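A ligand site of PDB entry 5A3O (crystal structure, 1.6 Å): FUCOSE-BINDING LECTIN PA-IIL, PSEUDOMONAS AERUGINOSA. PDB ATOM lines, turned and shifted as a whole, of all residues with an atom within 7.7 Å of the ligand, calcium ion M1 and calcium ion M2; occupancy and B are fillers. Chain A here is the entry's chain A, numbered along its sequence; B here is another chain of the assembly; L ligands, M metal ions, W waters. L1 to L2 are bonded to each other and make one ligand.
The backbone NH of Ser 23 is in hydrogen-bond range of an oxygen (O5) of LIG L1 (3.0 Å).
O1 of LG2 L2 sits at hydrogen-bond distance from N of Gly 24 (3.3 Å).
An oxygen (O5) of LIG L1 sits close to the side-chain hydroxyl (OG) of Ser 23, at 3.4 Å.
An oxygen (O4) of LIG L1 lies close to the side-chain carboxylate of Asp 96 (2.6 Å).
CA of Ser 22 touches O2 of LIG L1 (3.3 Å).
CA of Gly 97 touches O4 of LIG L1, 3.98 Å away.
Of the 26 residues printed, 11 come within 4 Å of the ligand.
Calcium ion M1 is bound by OD1 of Asp 101 (2.3 Å), OD1 of Asp 99 (2.4 Å), O3 of LIG L1 (2.4 Å), OD2 of Asp 104 (2.4 Å), OE2 of Glu 95 (2.5 Å), OE1 of Glu 95 (2.5 Å), O4 of LIG L1 (2.7 Å) and OD1 of Asp 104 (2.7 Å).
The side-chain carboxylate (OD2) of Asp 96 lies within hydrogen-bond range of the side-chain hydroxyl (OG) of Ser 22 (2.6 Å).
NE2 of Gln 26 is in hydrogen-bond range of OD2 of Asp 96 (3.1 Å).
The side-chain carboxylate (OE1) of Glu 95 sits close to the backbone NH (N) of Asn 100 (3.3 Å).
The backbone NH of Asn 103 sits at hydrogen-bond distance from the backbone carbonyl oxygen of Ser 94, 3.4 Å away.
The backbone carbonyl oxygen (O) of Pro 112 of chain B is in hydrogen-bond range of the side-chain amide nitrogen (ND2) of Asn 103, at 2.7 Å.
OG of Ser 22 is in hydrogen-bond range of N of Gly 24.
The backbone NH of Ser 22 sits at hydrogen-bond distance from the backbone carbonyl oxygen of Ser 44.
The side-chain carboxylate (OD2) of Asp 104 lies close to the backbone NH (N) of Asp 96, at 2.8 Å.
Asp 96 touches calcium ion M1.
Within 4 Å of calcium ion M1: Glu 95, Asp 96, Asp 99, Asp 101 and Asp 104.
The nearest printed residue that does not touch calcium ion M1 is Tyr 102 (4.4 Å).
Water W4 lies within hydrogen-bond range of an oxygen (O1) of LG2 L2 (2.8 Å) and the side-chain carboxylate of Asp 96 (3.0 Å).
Water W6 lies within hydrogen-bond range of O1 of LG2 L2, N of Gly 24 and O of Ser 23.
Water W2 bridges O1 of LIG L1 (3.3 Å) and OD2 of Asp 99 (3.3 Å).
Calcium ion M2 is bound by the side-chain amide oxygen of Asn 103 (2.3 Å), the backbone carbonyl oxygen of Asn 21 (2.3 Å), the side-chain carboxylate of Asp 104 (2.3 Å), the side-chain carboxylate of Asp 101 (2.4 Å), the chain-end carboxylate of Gly 114 of chain B (2.4 Å), an oxygen (O2) of LIG L1 (2.5 Å) and an oxygen (O3) of LIG L1 (2.5 Å).
Calcium ion M2 has seven donor atoms within binding distance.
Slightly farther from calcium ion M2 lies the side-chain carboxylate (OD1) of Asp 101 (3.0 Å).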
ATOM      1  N   ALA A  20       9.122  23.065  -5.995  1.00  0.00           N
ATOM      2  CA  ALA A  20      10.345  22.243  -6.202  1.00  0.00           C
ATOM      3  C   ALA A  20      10.796  21.504  -4.967  1.00  0.00           C
ATOM      4  O   ALA A  20      10.830  22.089  -3.873  1.00  0.00           O
ATOM      5  CB  ALA A  20      11.495  23.138  -6.692  1.00  0.00           C
ATOM      6  N   ASN A  21      11.223  20.253  -5.193  1.00  0.00           N
ATOM      7  CA  ASN A  21      11.788  19.375  -4.153  1.00  0.00           C
ATOM      8  C   ASN A  21      12.872  18.512  -4.723  1.00  0.00           C
ATOM      9  O   ASN A  21      12.690  17.309  -4.947  1.00  0.00           O
ATOM     10  CB  ASN A  21      10.690  18.512  -3.530  1.00  0.00           C
ATOM     11  CG  ASN A  21       9.717  19.314  -2.714  1.00  0.00           C
ATOM     12  OD1 ASN A  21      10.020  19.733  -1.572  1.00  0.00           O
ATOM     13  ND2 ASN A  21       8.524  19.496  -3.239  1.00  0.00           N
ATOM     14  N   SER A  22      14.001  19.134  -5.003  1.00  0.00           N
ATOM     15  CA  SER A  22      15.105  18.445  -5.641  1.00  0.00           C
ATOM     16  C   SER A  22      16.367  19.203  -5.566  1.00  0.00           C
ATOM     17  O   SER A  22      16.375  20.403  -5.466  1.00  0.00           O
ATOM     18  CB  SER A  22      14.772  18.209  -7.126  1.00  0.00           C
ATOM     19  OG  SER A  22      15.843  17.553  -7.831  1.00  0.00           O
ATOM     20  N   SER A  23      17.460  18.464  -5.629  1.00  0.00           N
ATOM     21  CA  SER A  23      18.770  19.107  -5.756  1.00  0.00           C
ATOM     22  C   SER A  23      18.941  19.844  -7.113  1.00  0.00           C
ATOM     23  O   SER A  23      19.739  20.799  -7.219  1.00  0.00           O
ATOM     24  CB  SER A  23      19.881  18.096  -5.599  1.00  0.00           C
ATOM     25  OG  SER A  23      20.032  17.678  -4.243  1.00  0.00           O
ATOM     26  N   GLY A  24      18.252  19.384  -8.152  1.00  0.00           N
ATOM     27  CA  GLY A  24      18.353  19.996  -9.461  1.00  0.00           C
ATOM     28  C   GLY A  24      17.374  21.135  -9.710  1.00  0.00           C
ATOM     29  O   GLY A  24      16.229  21.108  -9.237  1.00  0.00           O
ATOM     30  N   THR A  25      17.790  22.117 -10.509  1.00  0.00           N
ATOM     31  CA  THR A  25      16.884  23.182 -10.922  1.00  0.00           C
ATOM     32  C   THR A  25      15.812  22.635 -11.865  1.00  0.00           C
ATOM     33  O   THR A  25      16.092  22.017 -12.899  1.00  0.00           O
ATOM     34  CB  THR A  25      17.645  24.317 -11.627  1.00  0.00           C
ATOM     35  OG1 THR A  25      18.695  24.777 -10.758  1.00  0.00           O
ATOM     36  CG2 THR A  25      16.694  25.474 -12.058  1.00  0.00           C
ATOM     37  N   GLN A  26      14.576  22.889 -11.491  1.00  0.00           N
ATOM     38  CA  GLN A  26      13.421  22.456 -12.300  1.00  0.00           C
ATOM     39  C   GLN A  26      13.018  23.528 -13.281  1.00  0.00           C
ATOM     40  O   GLN A  26      13.126  24.743 -12.972  1.00  0.00           O
ATOM     41  CB  GLN A  26      12.234  22.156 -11.406  1.00  0.00           C
ATOM     42  CG  GLN A  26      12.588  21.223 -10.238  1.00  0.00           C
ATOM     43  CD  GLN A  26      12.903  19.807 -10.704  1.00  0.00           C
ATOM     44  OE1 GLN A  26      12.104  19.228 -11.414  1.00  0.00           O
ATOM     45  NE2 GLN A  26      14.075  19.271 -10.318  1.00  0.00           N
ATOM     46  N   GLN A  43      15.144  26.038  -7.806  1.00  0.00           N
ATOM     47  CA  GLN A  43      15.788  24.929  -7.185  1.00  0.00           C
ATOM     48  C   GLN A  43      15.559  25.018  -5.687  1.00  0.00           C
ATOM     49  O   GLN A  43      16.005  25.978  -5.039  1.00  0.00           O
ATOM     50  CB  GLN A  43      17.297  24.880  -7.509  1.00  0.00           C
ATOM     51  CG  GLN A  43      18.022  23.632  -6.994  1.00  0.00           C
ATOM     52  CD  GLN A  43      18.403  23.718  -5.505  1.00  0.00           C
ATOM     53  OE1 GLN A  43      19.016  24.707  -5.096  1.00  0.00           O
ATOM     54  NE2 GLN A  43      18.040  22.697  -4.709  1.00  0.00           N
ATOM     55  N   SER A  44      14.921  23.996  -5.125  1.00  0.00           N
ATOM     56  CA  SER A  44      14.643  23.934  -3.696  1.00  0.00           C
ATOM     57  C   SER A  44      14.441  22.490  -3.305  1.00  0.00           C
ATOM     58  O   SER A  44      13.923  21.712  -4.108  1.00  0.00           O
ATOM     59  CB  SER A  44      13.379  24.727  -3.394  1.00  0.00           C
ATOM     60  OG  SER A  44      12.975  24.644  -2.028  1.00  0.00           O
ATOM     61  N   THR A  45      14.843  22.107  -2.101  1.00  0.00           N
ATOM     62  CA  THR A  45      14.482  20.826  -1.512  1.00  0.00           C
ATOM     63  C   THR A  45      13.491  21.018  -0.360  1.00  0.00           C
ATOM     64  O   THR A  45      13.292  20.101   0.467  1.00  0.00           O
ATOM     65  CB  THR A  45      15.710  20.038  -1.001  1.00  0.00           C
ATOM     66  OG1 THR A  45      16.409  20.812  -0.016  1.00  0.00           O
ATOM     67  CG2 THR A  45      16.613  19.653  -2.134  1.00  0.00           C
ATOM     68  N   VAL A  69      14.756  19.033 -16.391  1.00  0.00           N
ATOM     69  CA  VAL A  69      15.867  19.546 -15.607  1.00  0.00           C
ATOM     70  C   VAL A  69      17.049  19.660 -16.553  1.00  0.00           C
ATOM     71  O   VAL A  69      17.516  18.654 -17.080  1.00  0.00           O
ATOM     72  CB  VAL A  69      16.221  18.625 -14.447  1.00  0.00           C
ATOM     73  CG1 VAL A  69      17.481  19.112 -13.769  1.00  0.00           C
ATOM     74  CG2 VAL A  69      15.075  18.579 -13.433  1.00  0.00           C
ATOM     75  N   SER A  94       6.449  14.775 -10.789  1.00  0.00           N
ATOM     76  CA  SER A  94       7.543  14.527 -11.724  1.00  0.00           C
ATOM     77  C   SER A  94       8.759  13.970 -11.000  1.00  0.00           C
ATOM     78  O   SER A  94       9.003  14.283  -9.836  1.00  0.00           O
ATOM     79  CB  SER A  94       7.917  15.747 -12.547  1.00  0.00           C
ATOM     80  OG  SER A  94       8.437  16.796 -11.756  1.00  0.00           O
ATOM     81  N   GLU A  95       9.477  13.116 -11.720  1.00  0.00           N
ATOM     82  CA  GLU A  95      10.683  12.474 -11.182  1.00  0.00           C
ATOM     83  C   GLU A  95      11.814  12.750 -12.125  1.00  0.00           C
ATOM     84  O   GLU A  95      11.749  12.448 -13.334  1.00  0.00           O
ATOM     85  CB  GLU A  95      10.467  10.964 -11.084  1.00  0.00           C
ATOM     86  CG  GLU A  95      11.659  10.206 -10.548  1.00  0.00           C
ATOM     87  CD  GLU A  95      12.224  10.796  -9.272  1.00  0.00           C
ATOM     88  OE1 GLU A  95      11.455  10.938  -8.291  1.00  0.00           O
ATOM     89  OE2 GLU A  95      13.476  11.038  -9.180  1.00  0.00           O
ATOM     90  N   ASP A  96      12.861  13.356 -11.582  1.00  0.00           N
ATOM     91  CA  ASP A  96      14.050  13.682 -12.348  1.00  0.00           C
ATOM     92  C   ASP A  96      15.203  12.714 -12.137  1.00  0.00           C
ATOM     93  O   ASP A  96      16.289  12.946 -12.701  1.00  0.00           O
ATOM     94  CB  ASP A  96      14.493  15.113 -11.990  1.00  0.00           C
ATOM     95  CG  ASP A  96      15.019  15.251 -10.557  1.00  0.00           C
ATOM     96  OD1 ASP A  96      15.283  14.224  -9.875  1.00  0.00           O
ATOM     97  OD2 ASP A  96      15.120  16.412 -10.057  1.00  0.00           O
ATOM     98  N   GLY A  97      15.003  11.665 -11.353  1.00  0.00           N
ATOM     99  CA  GLY A  97      16.131  10.906 -10.823  1.00  0.00           C
ATOM    100  C   GLY A  97      15.810   9.437 -10.672  1.00  0.00           C
ATOM    101  O   GLY A  97      15.071   8.877 -11.482  1.00  0.00           O
ATOM    102  N   THR A  98      16.359   8.861  -9.631  1.00  0.00           N
ATOM    103  CA  THR A  98      16.227   7.430  -9.311  1.00  0.00           C
ATOM    104  C   THR A  98      15.388   7.075  -8.090  1.00  0.00           C
ATOM    105  O   THR A  98      15.027   5.898  -7.913  1.00  0.00           O
ATOM    106  CB  THR A  98      17.641   6.846  -9.107  1.00  0.00           C
ATOM    107  OG1 THR A  98      18.317   7.515  -8.047  1.00  0.00           O
ATOM    108  CG2 THR A  98      18.442   7.085 -10.325  1.00  0.00           C
ATOM    109  N   ASP A  99      15.113   8.051  -7.218  1.00  0.00           N
ATOM    110  CA  ASP A  99      14.438   7.742  -5.951  1.00  0.00           C
ATOM    111  C   ASP A  99      12.911   7.588  -6.043  1.00  0.00           C
ATOM    112  O   ASP A  99      12.298   7.129  -5.070  1.00  0.00           O
ATOM    113  CB  ASP A  99      14.823   8.707  -4.827  1.00  0.00           C
ATOM    114  CG  ASP A  99      14.260  10.098  -4.990  1.00  0.00           C
ATOM    115  OD1 ASP A  99      13.685  10.348  -6.049  1.00  0.00           O
ATOM    116  OD2 ASP A  99      14.421  10.896  -4.038  1.00  0.00           O
ATOM    117  N   ASN A 100      12.320   7.976  -7.174  1.00  0.00           N
ATOM    118  CA  ASN A 100      10.893   7.866  -7.384  1.00  0.00           C
ATOM    119  C   ASN A 100      10.058   8.466  -6.285  1.00  0.00           C
ATOM    120  O   ASN A 100       8.993   7.906  -5.906  1.00  0.00           O
ATOM    121  CB  ASN A 100      10.500   6.426  -7.651  1.00  0.00           C
ATOM    122  CG  ASN A 100      11.136   5.906  -8.912  1.00  0.00           C
ATOM    123  OD1 ASN A 100      11.486   6.690  -9.789  1.00  0.00           O
ATOM    124  ND2 ASN A 100      11.265   4.600  -9.012  1.00  0.00           N
ATOM    125  N   ASP A 101      10.524   9.617  -5.791  1.00  0.00           N
ATOM    126  CA  ASP A 101       9.674  10.407  -4.899  1.00  0.00           C
ATOM    127  C   ASP A 101       8.620  11.198  -5.677  1.00  0.00           C
ATOM    128  O   ASP A 101       7.602  11.585  -5.089  1.00  0.00           O
ATOM    129  CB  ASP A 101      10.425  11.229  -3.852  1.00  0.00           C
ATOM    130  CG  ASP A 101      11.254  12.330  -4.387  1.00  0.00           C
ATOM    131  OD1 ASP A 101      11.401  12.516  -5.601  1.00  0.00           O
ATOM    132  OD2 ASP A 101      11.770  13.037  -3.521  1.00  0.00           O
ATOM    133  N   TYR A 102       8.855  11.421  -6.952  1.00  0.00           N
ATOM    134  CA  TYR A 102       7.887  12.095  -7.843  1.00  0.00           C
ATOM    135  C   TYR A 102       7.407  13.472  -7.380  1.00  0.00           C
ATOM    136  O   TYR A 102       6.348  13.953  -7.833  1.00  0.00           O
ATOM    137  CB  TYR A 102       6.683  11.153  -8.198  1.00  0.00           C
ATOM    138  CG  TYR A 102       7.061  10.263  -9.330  1.00  0.00           C
ATOM    139  CD1 TYR A 102       7.739   9.056  -9.090  1.00  0.00           C
ATOM    140  CD2 TYR A 102       6.814  10.640 -10.661  1.00  0.00           C
ATOM    141  CE1 TYR A 102       8.160   8.263 -10.132  1.00  0.00           C
ATOM    142  CE2 TYR A 102       7.233   9.838 -11.731  1.00  0.00           C
ATOM    143  CZ  TYR A 102       7.919   8.670 -11.441  1.00  0.00           C
ATOM    144  OH  TYR A 102       8.336   7.831 -12.448  1.00  0.00           O
ATOM    145  N   ASN A 103       8.238  14.143  -6.574  1.00  0.00           N
ATOM    146  CA  ASN A 103       7.945  15.488  -6.063  1.00  0.00           C
ATOM    147  C   ASN A 103       8.938  16.511  -6.554  1.00  0.00           C
ATOM    148  O   ASN A 103       8.954  17.637  -6.035  1.00  0.00           O
ATOM    149  CB  ASN A 103       7.962  15.523  -4.505  1.00  0.00           C
ATOM    150  CG  ASN A 103       9.373  15.394  -3.943  1.00  0.00           C
ATOM    151  OD1 ASN A 103      10.341  15.247  -4.691  1.00  0.00           O
ATOM    152  ND2 ASN A 103       9.501  15.421  -2.651  1.00  0.00           N
ATOM    153  N   ASP A 104       9.760  16.149  -7.553  1.00  0.00           N
ATOM    154  CA  ASP A 104      10.929  16.966  -7.842  1.00  0.00           C
ATOM    155  C   ASP A 104      10.457  18.342  -8.366  1.00  0.00           C
ATOM    156  O   ASP A 104      11.001  19.403  -8.006  1.00  0.00           O
ATOM    157  CB  ASP A 104      11.828  16.224  -8.814  1.00  0.00           C
ATOM    158  CG  ASP A 104      12.424  14.993  -8.199  1.00  0.00           C
ATOM    159  OD1 ASP A 104      12.682  15.044  -6.950  1.00  0.00           O
ATOM    160  OD2 ASP A 104      12.496  13.922  -8.901  1.00  0.00           O
ATOM    161  N   ALA A 105       9.454  18.274  -9.228  1.00  0.00           N
ATOM    162  CA  ALA A 105       8.539  19.401  -9.450  1.00  0.00           C
ATOM    163  C   ALA A 105       7.110  18.932  -9.306  1.00  0.00           C
ATOM    164  O   ALA A 105       6.714  17.941  -9.885  1.00  0.00           O
ATOM    165  CB  ALA A 105       8.707  20.026 -10.816  1.00  0.00           C
ATOM    166  N   PRO B 112       5.652  13.578   0.155  1.00  0.00           N
ATOM    167  CA  PRO B 112       6.833  14.080   0.895  1.00  0.00           C
ATOM    168  C   PRO B 112       7.470  15.265   0.249  1.00  0.00           C
ATOM    169  O   PRO B 112       7.314  15.511  -1.010  1.00  0.00           O
ATOM    170  CB  PRO B 112       7.780  12.864   0.807  1.00  0.00           C
ATOM    171  CG  PRO B 112       7.459  12.285  -0.522  1.00  0.00           C
ATOM    172  CD  PRO B 112       5.959  12.365  -0.610  1.00  0.00           C
ATOM    173  N   LEU B 113       8.280  15.957   1.052  1.00  0.00           N
ATOM    174  CA  LEU B 113       9.162  16.995   0.543  1.00  0.00           C
ATOM    175  C   LEU B 113      10.580  16.445   0.315  1.00  0.00           C
ATOM    176  O   LEU B 113      10.901  15.287   0.611  1.00  0.00           O
ATOM    177  CB  LEU B 113       9.141  18.181   1.521  1.00  0.00           C
ATOM    178  CG  LEU B 113       7.757  18.740   1.860  1.00  0.00           C
ATOM    179  CD1 LEU B 113       7.872  19.961   2.781  1.00  0.00           C
ATOM    180  CD2 LEU B 113       6.969  19.126   0.595  1.00  0.00           C
ATOM    181  N   GLY B 114      11.469  17.285  -0.181  1.00  0.00           N
ATOM    182  CA  GLY B 114      12.891  16.972  -0.244  1.00  0.00           C
ATOM    183  C   GLY B 114      13.332  16.422  -1.560  1.00  0.00           C
ATOM    184  O   GLY B 114      12.552  15.800  -2.289  1.00  0.00           O
ATOM    185  OXT GLY B 114      14.520  16.575  -1.865  1.00  0.00           O
HETATM  186  C1  LIG L   1      17.402  15.047  -4.111  1.00  0.00           C
HETATM  187  C2  LIG L   1      15.984  14.488  -4.066  1.00  0.00           C
HETATM  188  C3  LIG L   1      15.664  13.499  -5.170  1.00  0.00           C
HETATM  189  C4  LIG L   1      16.009  14.065  -6.518  1.00  0.00           C
HETATM  190  C5  LIG L   1      17.491  14.448  -6.451  1.00  0.00           C
HETATM  191  C6  LIG L   1      18.031  14.998  -7.751  1.00  0.00           C
HETATM  192  C7  LIG L   1      19.613  14.451  -3.507  1.00  0.00           C
HETATM  193  O1  LIG L   1      18.280  13.966  -3.765  1.00  0.00           O
HETATM  194  O2  LIG L   1      15.038  15.533  -4.171  1.00  0.00           O
HETATM  195  O3  LIG L   1      14.259  13.184  -5.158  1.00  0.00           O
HETATM  196  O4  LIG L   1      15.717  13.101  -7.527  1.00  0.00           O
HETATM  197  O5  LIG L   1      17.675  15.480  -5.453  1.00  0.00           O
HETATM  198  C1  LG2 L   2      20.350  15.564  -8.259  1.00  0.00           C
HETATM  199  N1  LG2 L   2      19.475  14.779  -7.684  1.00  0.00           N
HETATM  200  O1  LG2 L   2      19.990  16.599  -8.816  1.00  0.00           O
HETATM  201  C2  LG2 L   2      21.785  15.228  -8.236  1.00  0.00           C
HETATM  202  C3  LG2 L   2      22.643  15.985  -8.955  1.00  0.00           C
HETATM  203  C4  LG2 L   2      24.073  15.642  -9.167  1.00  0.00           C
HETATM  204  C5  LG2 L   2      24.877  16.519  -9.913  1.00  0.00           C
HETATM  205  C6  LG2 L   2      26.233  16.225 -10.089  1.00  0.00           C
HETATM  206  C7  LG2 L   2      26.751  15.083  -9.510  1.00  0.00           C
HETATM  207  C8  LG2 L   2      25.961  14.232  -8.763  1.00  0.00           C
HETATM  208  C9  LG2 L   2      24.628  14.513  -8.570  1.00  0.00           C
HETATM  209 CA    CA M   1      13.165  12.405  -7.143  1.00  0.00          CA
HETATM  210 CA    CA M   2      12.645  15.016  -4.608  1.00  0.00          CA
HETATM  211  O   HOH W   1      21.018  12.758  -5.925  1.00  0.00           O
HETATM  212  O   HOH W   2      17.282  11.171  -2.318  1.00  0.00           O
HETATM  213  O   HOH W   3      16.729  10.620  -7.260  1.00  0.00           O
HETATM  214  O   HOH W   4      18.007  16.976 -10.792  1.00  0.00           O
HETATM  215  O   HOH W   5      22.429  16.476  -3.082  1.00  0.00           O
HETATM  216  O   HOH W   6      21.258  18.981  -9.669  1.00  0.00           O
